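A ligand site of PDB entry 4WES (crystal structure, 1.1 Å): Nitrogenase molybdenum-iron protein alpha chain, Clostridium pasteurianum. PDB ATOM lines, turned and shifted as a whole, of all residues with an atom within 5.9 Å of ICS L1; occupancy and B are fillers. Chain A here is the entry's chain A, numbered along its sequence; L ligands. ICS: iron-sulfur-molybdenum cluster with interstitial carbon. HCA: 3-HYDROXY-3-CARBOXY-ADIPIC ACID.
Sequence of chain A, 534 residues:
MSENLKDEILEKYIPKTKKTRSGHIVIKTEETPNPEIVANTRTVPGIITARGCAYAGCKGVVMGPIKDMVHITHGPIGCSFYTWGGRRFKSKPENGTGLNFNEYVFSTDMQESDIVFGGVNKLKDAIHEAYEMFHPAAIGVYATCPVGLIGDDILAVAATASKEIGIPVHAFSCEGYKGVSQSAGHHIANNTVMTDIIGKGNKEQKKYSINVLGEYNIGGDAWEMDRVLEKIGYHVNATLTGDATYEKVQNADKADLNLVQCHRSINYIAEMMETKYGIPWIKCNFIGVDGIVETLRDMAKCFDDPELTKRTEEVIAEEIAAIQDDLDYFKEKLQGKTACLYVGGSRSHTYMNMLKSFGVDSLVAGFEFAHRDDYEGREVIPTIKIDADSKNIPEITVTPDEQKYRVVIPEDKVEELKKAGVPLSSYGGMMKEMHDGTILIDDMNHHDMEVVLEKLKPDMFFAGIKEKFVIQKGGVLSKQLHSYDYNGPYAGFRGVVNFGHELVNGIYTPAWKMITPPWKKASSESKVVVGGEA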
ATOM      1  N   GLY A  57      -4.617   6.984  19.730  1.00  0.00           N
ATOM      2  CA  GLY A  57      -4.595   8.375  20.154  1.00  0.00           C
ATOM      3  C   GLY A  57      -3.569   9.233  19.427  1.00  0.00           C
ATOM      4  O   GLY A  57      -3.763  10.431  19.201  1.00  0.00           O
ATOM      5  N   VAL A  61      -5.726   9.667  15.795  1.00  0.00           N
ATOM      6  CA  VAL A  61      -6.436  10.828  16.311  1.00  0.00           C
ATOM      7  C   VAL A  61      -5.673  12.125  16.036  1.00  0.00           C
ATOM      8  O   VAL A  61      -6.096  12.927  15.210  1.00  0.00           O
ATOM      9  CB  VAL A  61      -6.809  10.648  17.811  1.00  0.00           C
ATOM     10  CG1 VAL A  61      -7.378  11.932  18.386  1.00  0.00           C
ATOM     11  CG2 VAL A  61      -7.779   9.471  17.948  1.00  0.00           C
ATOM     12  N   VAL A  62      -4.539  12.364  16.696  1.00  0.00           N
ATOM     13  CA  VAL A  62      -3.916  13.670  16.566  1.00  0.00           C
ATOM     14  C   VAL A  62      -3.203  13.879  15.246  1.00  0.00           C
ATOM     15  O   VAL A  62      -3.315  14.941  14.609  1.00  0.00           O
ATOM     16  CB  VAL A  62      -2.974  13.950  17.771  1.00  0.00           C
ATOM     17  CG1 VAL A  62      -2.213  15.265  17.566  1.00  0.00           C
ATOM     18  CG2 VAL A  62      -3.781  14.000  19.055  1.00  0.00           C
ATOM     19  N   ARG A  87     -12.358   7.148  11.175  1.00  0.00           N
ATOM     20  CA  ARG A  87     -12.454   8.419  11.887  1.00  0.00           C
ATOM     21  C   ARG A  87     -12.530   9.510  10.811  1.00  0.00           C
ATOM     22  O   ARG A  87     -11.656   9.626   9.961  1.00  0.00           O
ATOM     23  CB  ARG A  87     -11.284   8.629  12.822  1.00  0.00           C
ATOM     24  CG  ARG A  87     -11.357   9.952  13.567  1.00  0.00           C
ATOM     25  CD  ARG A  87     -10.473   9.971  14.753  1.00  0.00           C
ATOM     26  NE  ARG A  87     -10.361  11.269  15.395  1.00  0.00           N
ATOM     27  CZ  ARG A  87      -9.442  12.198  15.102  1.00  0.00           C
ATOM     28  NH1 ARG A  87      -9.376  13.309  15.814  1.00  0.00           N
ATOM     29  NH2 ARG A  87      -8.579  12.016  14.100  1.00  0.00           N
ATOM     30  N   GLN A 182      -6.271   5.776  24.806  1.00  0.00           N
ATOM     31  CA  GLN A 182      -5.884   6.735  23.760  1.00  0.00           C
ATOM     32  C   GLN A 182      -5.122   7.932  24.307  1.00  0.00           C
ATOM     33  O   GLN A 182      -4.348   8.565  23.560  1.00  0.00           O
ATOM     34  CB  GLN A 182      -7.119   7.226  23.012  1.00  0.00           C
ATOM     35  CG  GLN A 182      -7.902   6.185  22.211  1.00  0.00           C
ATOM     36  CD  GLN A 182      -9.061   5.589  23.001  1.00  0.00           C
ATOM     37  OE1 GLN A 182      -8.878   5.136  24.112  1.00  0.00           O
ATOM     38  NE2 GLN A 182     -10.223   5.506  22.382  1.00  0.00           N
ATOM     39  N   HIS A 186      -2.200  10.918  22.709  1.00  0.00           N
ATOM     40  CA  HIS A 186      -2.277  12.357  22.561  1.00  0.00           C
ATOM     41  C   HIS A 186      -1.009  13.004  23.069  1.00  0.00           C
ATOM     42  O   HIS A 186      -0.419  13.886  22.431  1.00  0.00           O
ATOM     43  CB  HIS A 186      -3.399  12.970  23.390  1.00  0.00           C
ATOM     44  CG  HIS A 186      -4.777  12.448  23.129  1.00  0.00           C
ATOM     45  ND1 HIS A 186      -5.756  12.531  24.098  1.00  0.00           N
ATOM     46  CD2 HIS A 186      -5.328  11.856  22.050  1.00  0.00           C
ATOM     47  CE1 HIS A 186      -6.860  12.043  23.595  1.00  0.00           C
ATOM     48  NE2 HIS A 186      -6.638  11.601  22.376  1.00  0.00           N
ATOM     49  N   GLY A 214      -7.007  21.334  19.011  1.00  0.00           N
ATOM     50  CA  GLY A 214      -7.796  20.173  19.413  1.00  0.00           C
ATOM     51  C   GLY A 214      -9.133  20.140  18.704  1.00  0.00           C
ATOM     52  O   GLY A 214     -10.203  19.951  19.310  1.00  0.00           O
ATOM     53  N   TYR A 216     -10.576  18.505  14.877  1.00  0.00           N
ATOM     54  CA  TYR A 216     -10.095  17.546  13.883  1.00  0.00           C
ATOM     55  C   TYR A 216     -10.969  17.482  12.643  1.00  0.00           C
ATOM     56  O   TYR A 216     -10.804  16.617  11.802  1.00  0.00           O
ATOM     57  CB  TYR A 216      -9.849  16.202  14.565  1.00  0.00           C
ATOM     58  CG  TYR A 216      -8.919  16.367  15.731  1.00  0.00           C
ATOM     59  CD1 TYR A 216      -7.553  16.456  15.530  1.00  0.00           C
ATOM     60  CD2 TYR A 216      -9.401  16.483  17.016  1.00  0.00           C
ATOM     61  CE1 TYR A 216      -6.680  16.684  16.574  1.00  0.00           C
ATOM     62  CE2 TYR A 216      -8.533  16.690  18.083  1.00  0.00           C
ATOM     63  CZ  TYR A 216      -7.173  16.783  17.867  1.00  0.00           C
ATOM     64  OH  TYR A 216      -6.300  16.997  18.908  1.00  0.00           O
ATOM     65  N   ILE A 218     -14.041  16.668  12.130  1.00  0.00           N
ATOM     66  CA  ILE A 218     -14.906  15.508  11.944  1.00  0.00           C
ATOM     67  C   ILE A 218     -16.199  15.963  11.279  1.00  0.00           C
ATOM     68  O   ILE A 218     -16.847  16.893  11.734  1.00  0.00           O
ATOM     69  CB  ILE A 218     -15.185  14.820  13.274  1.00  0.00           C
ATOM     70  CG1 ILE A 218     -13.891  14.459  14.038  1.00  0.00           C
ATOM     71  CG2 ILE A 218     -16.085  13.601  13.059  1.00  0.00           C
ATOM     72  CD1 ILE A 218     -12.860  13.648  13.252  1.00  0.00           C
ATOM     73  N   CYS A 262     -10.972  20.629  22.145  1.00  0.00           N
ATOM     74  CA  CYS A 262     -10.734  19.422  22.920  1.00  0.00           C
ATOM     75  C   CYS A 262      -9.621  19.662  23.933  1.00  0.00           C
ATOM     76  O   CYS A 262      -8.434  19.705  23.558  1.00  0.00           O
ATOM     77  CB  CYS A 262     -10.358  18.236  22.033  1.00  0.00           C
ATOM     78  SG  CYS A 262      -9.976  16.830  23.053  1.00  0.00           S
ATOM     79  N   ARG A 264      -8.580  17.661  26.437  1.00  0.00           N
ATOM     80  CA  ARG A 264      -7.783  16.508  26.765  1.00  0.00           C
ATOM     81  C   ARG A 264      -6.637  16.286  25.772  1.00  0.00           C
ATOM     82  O   ARG A 264      -5.504  16.007  26.168  1.00  0.00           O
ATOM     83  CB  ARG A 264      -8.698  15.257  26.828  1.00  0.00           C
ATOM     84  CG  ARG A 264      -8.007  13.951  27.171  1.00  0.00           C
ATOM     85  CD  ARG A 264      -7.453  13.858  28.575  1.00  0.00           C
ATOM     86  NE  ARG A 264      -6.136  14.468  28.735  1.00  0.00           N
ATOM     87  CZ  ARG A 264      -5.752  15.309  29.687  1.00  0.00           C
ATOM     88  NH1 ARG A 264      -6.602  15.851  30.530  1.00  0.00           N
ATOM     89  NH2 ARG A 264      -4.483  15.664  29.720  1.00  0.00           N
ATOM     90  N   SER A 265      -6.944  16.353  24.457  1.00  0.00           N
ATOM     91  CA  SER A 265      -5.967  15.934  23.492  1.00  0.00           C
ATOM     92  C   SER A 265      -4.878  16.969  23.215  1.00  0.00           C
ATOM     93  O   SER A 265      -3.812  16.584  22.723  1.00  0.00           O
ATOM     94  CB  SER A 265      -6.598  15.571  22.150  1.00  0.00           C
ATOM     95  OG  SER A 265      -7.157  16.717  21.503  1.00  0.00           O
ATOM     96  N   VAL A 343     -18.661   9.421  25.735  1.00  0.00           N
ATOM     97  CA  VAL A 343     -17.712   9.569  24.619  1.00  0.00           C
ATOM     98  C   VAL A 343     -16.281   9.457  25.161  1.00  0.00           C
ATOM     99  O   VAL A 343     -16.077   8.865  26.218  1.00  0.00           O
ATOM    100  CB  VAL A 343     -17.972  10.841  23.752  1.00  0.00           C
ATOM    101  CG1 VAL A 343     -17.725  10.543  22.306  1.00  0.00           C
ATOM    102  CG2 VAL A 343     -19.410  11.334  23.915  1.00  0.00           C
ATOM    103  N   GLY A 344     -15.287   9.921  24.431  1.00  0.00           N
ATOM    104  CA  GLY A 344     -13.920   9.599  24.780  1.00  0.00           C
ATOM    105  C   GLY A 344     -13.281  10.492  25.834  1.00  0.00           C
ATOM    106  O   GLY A 344     -12.889  10.024  26.924  1.00  0.00           O
ATOM    107  N   GLY A 345     -13.138  11.774  25.504  1.00  0.00           N
ATOM    108  CA  GLY A 345     -12.460  12.673  26.360  1.00  0.00           C
ATOM    109  C   GLY A 345     -12.939  14.102  26.388  1.00  0.00           C
ATOM    110  O   GLY A 345     -12.461  14.874  27.223  1.00  0.00           O
ATOM    111  N   SER A 346     -13.859  14.492  25.491  1.00  0.00           N
ATOM    112  CA  SER A 346     -14.341  15.877  25.427  1.00  0.00           C
ATOM    113  C   SER A 346     -15.827  15.971  25.159  1.00  0.00           C
ATOM    114  O   SER A 346     -16.517  16.788  25.770  1.00  0.00           O
ATOM    115  CB  SER A 346     -13.544  16.639  24.368  1.00  0.00           C
ATOM    116  OG  SER A 346     -14.014  17.941  24.143  1.00  0.00           O
ATOM    117  N   ARG A 347     -16.345  15.187  24.216  1.00  0.00           N
ATOM    118  CA  ARG A 347     -17.669  15.484  23.653  1.00  0.00           C
ATOM    119  C   ARG A 347     -18.831  15.233  24.612  1.00  0.00           C
ATOM    120  O   ARG A 347     -19.908  15.807  24.452  1.00  0.00           O
ATOM    121  CB  ARG A 347     -17.845  14.736  22.328  1.00  0.00           C
ATOM    122  CG  ARG A 347     -16.984  15.374  21.251  1.00  0.00           C
ATOM    123  CD  ARG A 347     -17.133  14.632  19.940  1.00  0.00           C
ATOM    124  NE  ARG A 347     -16.277  15.279  18.939  1.00  0.00           N
ATOM    125  CZ  ARG A 347     -16.106  14.820  17.720  1.00  0.00           C
ATOM    126  NH1 ARG A 347     -16.768  13.782  17.286  1.00  0.00           N
ATOM    127  NH2 ARG A 347     -15.261  15.453  16.928  1.00  0.00           N
ATOM    128  N   SER A 348     -18.631  14.387  25.634  1.00  0.00           N
ATOM    129  CA  SER A 348     -19.664  14.234  26.666  1.00  0.00           C
ATOM    130  C   SER A 348     -20.018  15.566  27.290  1.00  0.00           C
ATOM    131  O   SER A 348     -21.156  15.765  27.728  1.00  0.00           O
ATOM    132  CB  SER A 348     -19.195  13.272  27.765  1.00  0.00           C
ATOM    133  OG  SER A 348     -18.705  12.088  27.184  1.00  0.00           O
ATOM    134  N   PHE A 367     -16.601   9.642  30.480  1.00  0.00           N
ATOM    135  CA  PHE A 367     -15.582   9.573  29.463  1.00  0.00           C
ATOM    136  C   PHE A 367     -14.862   8.253  29.511  1.00  0.00           C
ATOM    137  O   PHE A 367     -14.673   7.662  30.589  1.00  0.00           O
ATOM    138  CB  PHE A 367     -14.536  10.652  29.710  1.00  0.00           C
ATOM    139  CG  PHE A 367     -15.003  12.069  29.522  1.00  0.00           C
ATOM    140  CD1 PHE A 367     -15.425  12.544  28.279  1.00  0.00           C
ATOM    141  CD2 PHE A 367     -14.949  12.975  30.595  1.00  0.00           C
ATOM    142  CE1 PHE A 367     -15.772  13.883  28.103  1.00  0.00           C
ATOM    143  CE2 PHE A 367     -15.282  14.312  30.400  1.00  0.00           C
ATOM    144  CZ  PHE A 367     -15.696  14.756  29.165  1.00  0.00           C
ATOM    145  N   GLU A 368     -14.405   7.787  28.340  1.00  0.00           N
ATOM    146  CA  GLU A 368     -13.520   6.626  28.276  1.00  0.00           C
ATOM    147  C   GLU A 368     -12.216   6.871  29.002  1.00  0.00           C
ATOM    148  O   GLU A 368     -11.741   5.975  29.717  1.00  0.00           O
ATOM    149  CB  GLU A 368     -13.212   6.251  26.830  1.00  0.00           C
ATOM    150  CG  GLU A 368     -14.356   5.763  25.963  1.00  0.00           C
ATOM    151  CD  GLU A 368     -13.921   5.392  24.552  1.00  0.00           C
ATOM    152  OE1 GLU A 368     -14.858   5.280  23.673  1.00  0.00           O
ATOM    153  OE2 GLU A 368     -12.716   5.191  24.283  1.00  0.00           O
ATOM    154  N   PHE A 369     -11.579   8.020  28.745  1.00  0.00           N
ATOM    155  CA  PHE A 369     -10.146   8.134  29.077  1.00  0.00           C
ATOM    156  C   PHE A 369      -9.732   9.520  29.535  1.00  0.00           C
ATOM    157  O   PHE A 369      -8.541   9.807  29.654  1.00  0.00           O
ATOM    158  CB  PHE A 369      -9.299   7.701  27.845  1.00  0.00           C
ATOM    159  CG  PHE A 369      -9.665   8.447  26.578  1.00  0.00           C
ATOM    160  CD1 PHE A 369      -9.381   9.797  26.413  1.00  0.00           C
ATOM    161  CD2 PHE A 369     -10.320   7.777  25.562  1.00  0.00           C
ATOM    162  CE1 PHE A 369      -9.803  10.467  25.323  1.00  0.00           C
ATOM    163  CE2 PHE A 369     -10.723   8.452  24.426  1.00  0.00           C
ATOM    164  CZ  PHE A 369     -10.503   9.799  24.322  1.00  0.00           C
ATOM    165  N   LEU A 481     -21.748  10.043  18.962  1.00  0.00           N
ATOM    166  CA  LEU A 481     -21.088  11.342  19.104  1.00  0.00           C
ATOM    167  C   LEU A 481     -19.646  11.350  18.624  1.00  0.00           C
ATOM    168  O   LEU A 481     -19.017  12.418  18.664  1.00  0.00           O
ATOM    169  CB  LEU A 481     -21.217  11.901  20.521  1.00  0.00           C
ATOM    170  CG  LEU A 481     -22.575  12.481  20.848  1.00  0.00           C
ATOM    171  CD1 LEU A 481     -22.572  13.037  22.269  1.00  0.00           C
ATOM    172  CD2 LEU A 481     -23.019  13.573  19.877  1.00  0.00           C
ATOM    173  N   HIS A 482     -19.097  10.218  18.202  1.00  0.00           N
ATOM    174  CA  HIS A 482     -17.786  10.207  17.563  1.00  0.00           C
ATOM    175  C   HIS A 482     -17.952  10.423  16.054  1.00  0.00           C
ATOM    176  O   HIS A 482     -17.517  11.435  15.484  1.00  0.00           O
ATOM    177  CB  HIS A 482     -16.990   8.912  17.789  1.00  0.00           C
ATOM    178  CG  HIS A 482     -16.813   8.432  19.189  1.00  0.00           C
ATOM    179  ND1 HIS A 482     -15.582   8.371  19.815  1.00  0.00           N
ATOM    180  CD2 HIS A 482     -17.706   7.817  20.020  1.00  0.00           C
ATOM    181  CE1 HIS A 482     -15.732   7.720  20.958  1.00  0.00           C
ATOM    182  NE2 HIS A 482     -17.008   7.392  21.108  1.00  0.00           N
ATOM    183  N   SER A 483     -18.598   9.470  15.392  1.00  0.00           N
ATOM    184  CA  SER A 483     -18.748   9.481  13.952  1.00  0.00           C
ATOM    185  C   SER A 483     -19.894  10.315  13.428  1.00  0.00           C
ATOM    186  O   SER A 483     -20.056  10.477  12.202  1.00  0.00           O
ATOM    187  CB  SER A 483     -18.962   8.080  13.412  1.00  0.00           C
ATOM    188  OG  SER A 483     -20.279   7.635  13.770  1.00  0.00           O
HETATM  189 FE1  ICS L   1     -10.652  15.076  21.759  1.00  0.00          FE
HETATM  190 MO1  ICS L   1     -13.560   9.323  19.156  1.00  0.00          MO
HETATM  191 FE2  ICS L   1     -10.304  12.468  21.345  1.00  0.00          FE
HETATM  192 FE3  ICS L   1     -11.587  13.947  19.530  1.00  0.00          FE
HETATM  193 FE4  ICS L   1     -12.703  13.465  21.888  1.00  0.00          FE
HETATM  194 FE5  ICS L   1     -13.778  11.315  20.948  1.00  0.00          FE
HETATM  195 FE6  ICS L   1     -11.398  10.359  20.352  1.00  0.00          FE
HETATM  196 FE7  ICS L   1     -12.677  11.790  18.614  1.00  0.00          FE
HETATM  197  CX  ICS L   1     -12.091  12.262  20.487  1.00  0.00           C
HETATM  198  S1A ICS L   1     -10.900  13.400  23.320  1.00  0.00           S
HETATM  199  S1B ICS L   1     -13.005   9.251  21.427  1.00  0.00           S
HETATM  200  S2A ICS L   1      -9.391  14.161  20.130  1.00  0.00           S
HETATM  201  S2B ICS L   1      -9.389  10.449  21.217  1.00  0.00           S
HETATM  202  S3A ICS L   1     -14.648  12.621  22.568  1.00  0.00           S
HETATM  203  S3B ICS L   1     -11.495   9.931  18.180  1.00  0.00           S
HETATM  204  S4A ICS L   1     -12.699  15.477  20.787  1.00  0.00           S
HETATM  205  S4B ICS L   1     -14.810  11.293  18.973  1.00  0.00           S
HETATM  206  S5A ICS L   1     -12.205  13.570  17.414  1.00  0.00           S
HETATM  207  C1  HCA L   2     -10.614   5.766  18.482  1.00  0.00           C
HETATM  208  C2  HCA L   2     -11.418   6.357  17.318  1.00  0.00           C
HETATM  209  C3  HCA L   2     -12.882   6.653  17.656  1.00  0.00           C
HETATM  210  C4  HCA L   2     -13.755   5.378  17.610  1.00  0.00           C
HETATM  211  C5  HCA L   2     -15.229   5.808  17.697  1.00  0.00           C
HETATM  212  C6  HCA L   2     -16.258   4.811  18.129  1.00  0.00           C
HETATM  213  C7  HCA L   2     -13.440   7.641  16.642  1.00  0.00           C
HETATM  214  O1  HCA L   2     -10.989   5.960  19.645  1.00  0.00           O
HETATM  215  O2  HCA L   2      -9.581   5.137  18.203  1.00  0.00           O
HETATM  216  O3  HCA L   2     -17.383   4.819  17.533  1.00  0.00           O
HETATM  217  O4  HCA L   2     -15.997   4.014  19.050  1.00  0.00           O
HETATM  218  O5  HCA L   2     -14.003   8.667  17.079  1.00  0.00           O
HETATM  219  O6  HCA L   2     -13.373   7.364  15.433  1.00  0.00           O
HETATM  220  O7  HCA L   2     -12.989   7.202  18.963  1.00  0.00           O
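Val 61 touches ICS L1 (CG1 to S2A, 3.5 Å). Tyr 216 touches ICS L1. Ile 218 touches ICS L1. CG1 of Val 343 touches S3A of ICS L1 (3.7 Å). Phe 369 touches ICS L1. Hydrophobic or aromatic side chains within 4 Å of ICS L1: Val 61, His 186, Tyr 216, Ile 218, Val 343, Phe 369 and His 482. Of the 24 residues printed, 14 come within 4 Å of ICS L1. The nearest printed residue that does not touch ICS L1 is Gln 182 (4.3 Å).
The side-chain sulfur (SG) of Cys 262 binds an iron atom (FE1) of ICS L1 (2.3 Å). MO1 of ICS L1 is bound by ND1 of His 482 (2.3 Å). A ring nitrogen (NE2) of His 186 sits close to a sulfur (S2B) of ICS L1. S5A of ICS L1 sits close to NH1 of Arg 87 (3.3 Å). A sulfur (S3A) of ICS L1 lies close to the backbone NH (N) of Gly 344 (3.3 Å). The backbone NH (N) of Gly 345 sits close to a sulfur (S3A) of ICS L1 (3.4 Å). The backbone NH (N) of Arg 347 sits close to a sulfur (S3A) of ICS L1. The guanidinium group (NH1) of Arg 347 lies close to a sulfur (S4B) of ICS L1, 3.6 Å away. The backbone NH (N) of Ser 346 lies close to a sulfur (S3A) of ICS L1, 3.6 Å away. The side-chain hydroxyl of Ser 265 lies close to a sulfur (S2A) of ICS L1, 3.7 Å away. The side-chain amide nitrogen (NE2) of Gln 182 sits at hydrogen-bond distance from an oxygen (O1) of HCA L2 (2.9 Å).
An oxygen (O7) of HCA L2 is bound to a molybdenum atom (MO1) of ICS L1.
OG of Ser 265 sits close to SG of Cys 262, 3.2 Å away. The backbone NH (N) of Arg 264 sits close to the side-chain sulfur (SG) of Cys 262 (3.8 Å). The backbone carbonyl oxygen (O) of His 482 sits at hydrogen-bond distance from the guanidinium group (NH1) of Arg 347, at 3.1 Å. NH2 of Arg 87 is in hydrogen-bond range of O of Val 61 (2.9 Å). The backbone carbonyl oxygen (O) of Gly 344 sits at hydrogen-bond distance from the backbone NH (N) of Phe 369, at 3.0 Å. N of Glu 368 is in hydrogen-bond range of O of Gly 344 (3.1 Å). OH of Tyr 216 sits at hydrogen-bond distance from OG of Ser 265 (2.7 Å). The backbone carbonyl oxygen (O) of Leu 481 lies within hydrogen-bond range of the guanidinium group (NH1) of Arg 347.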
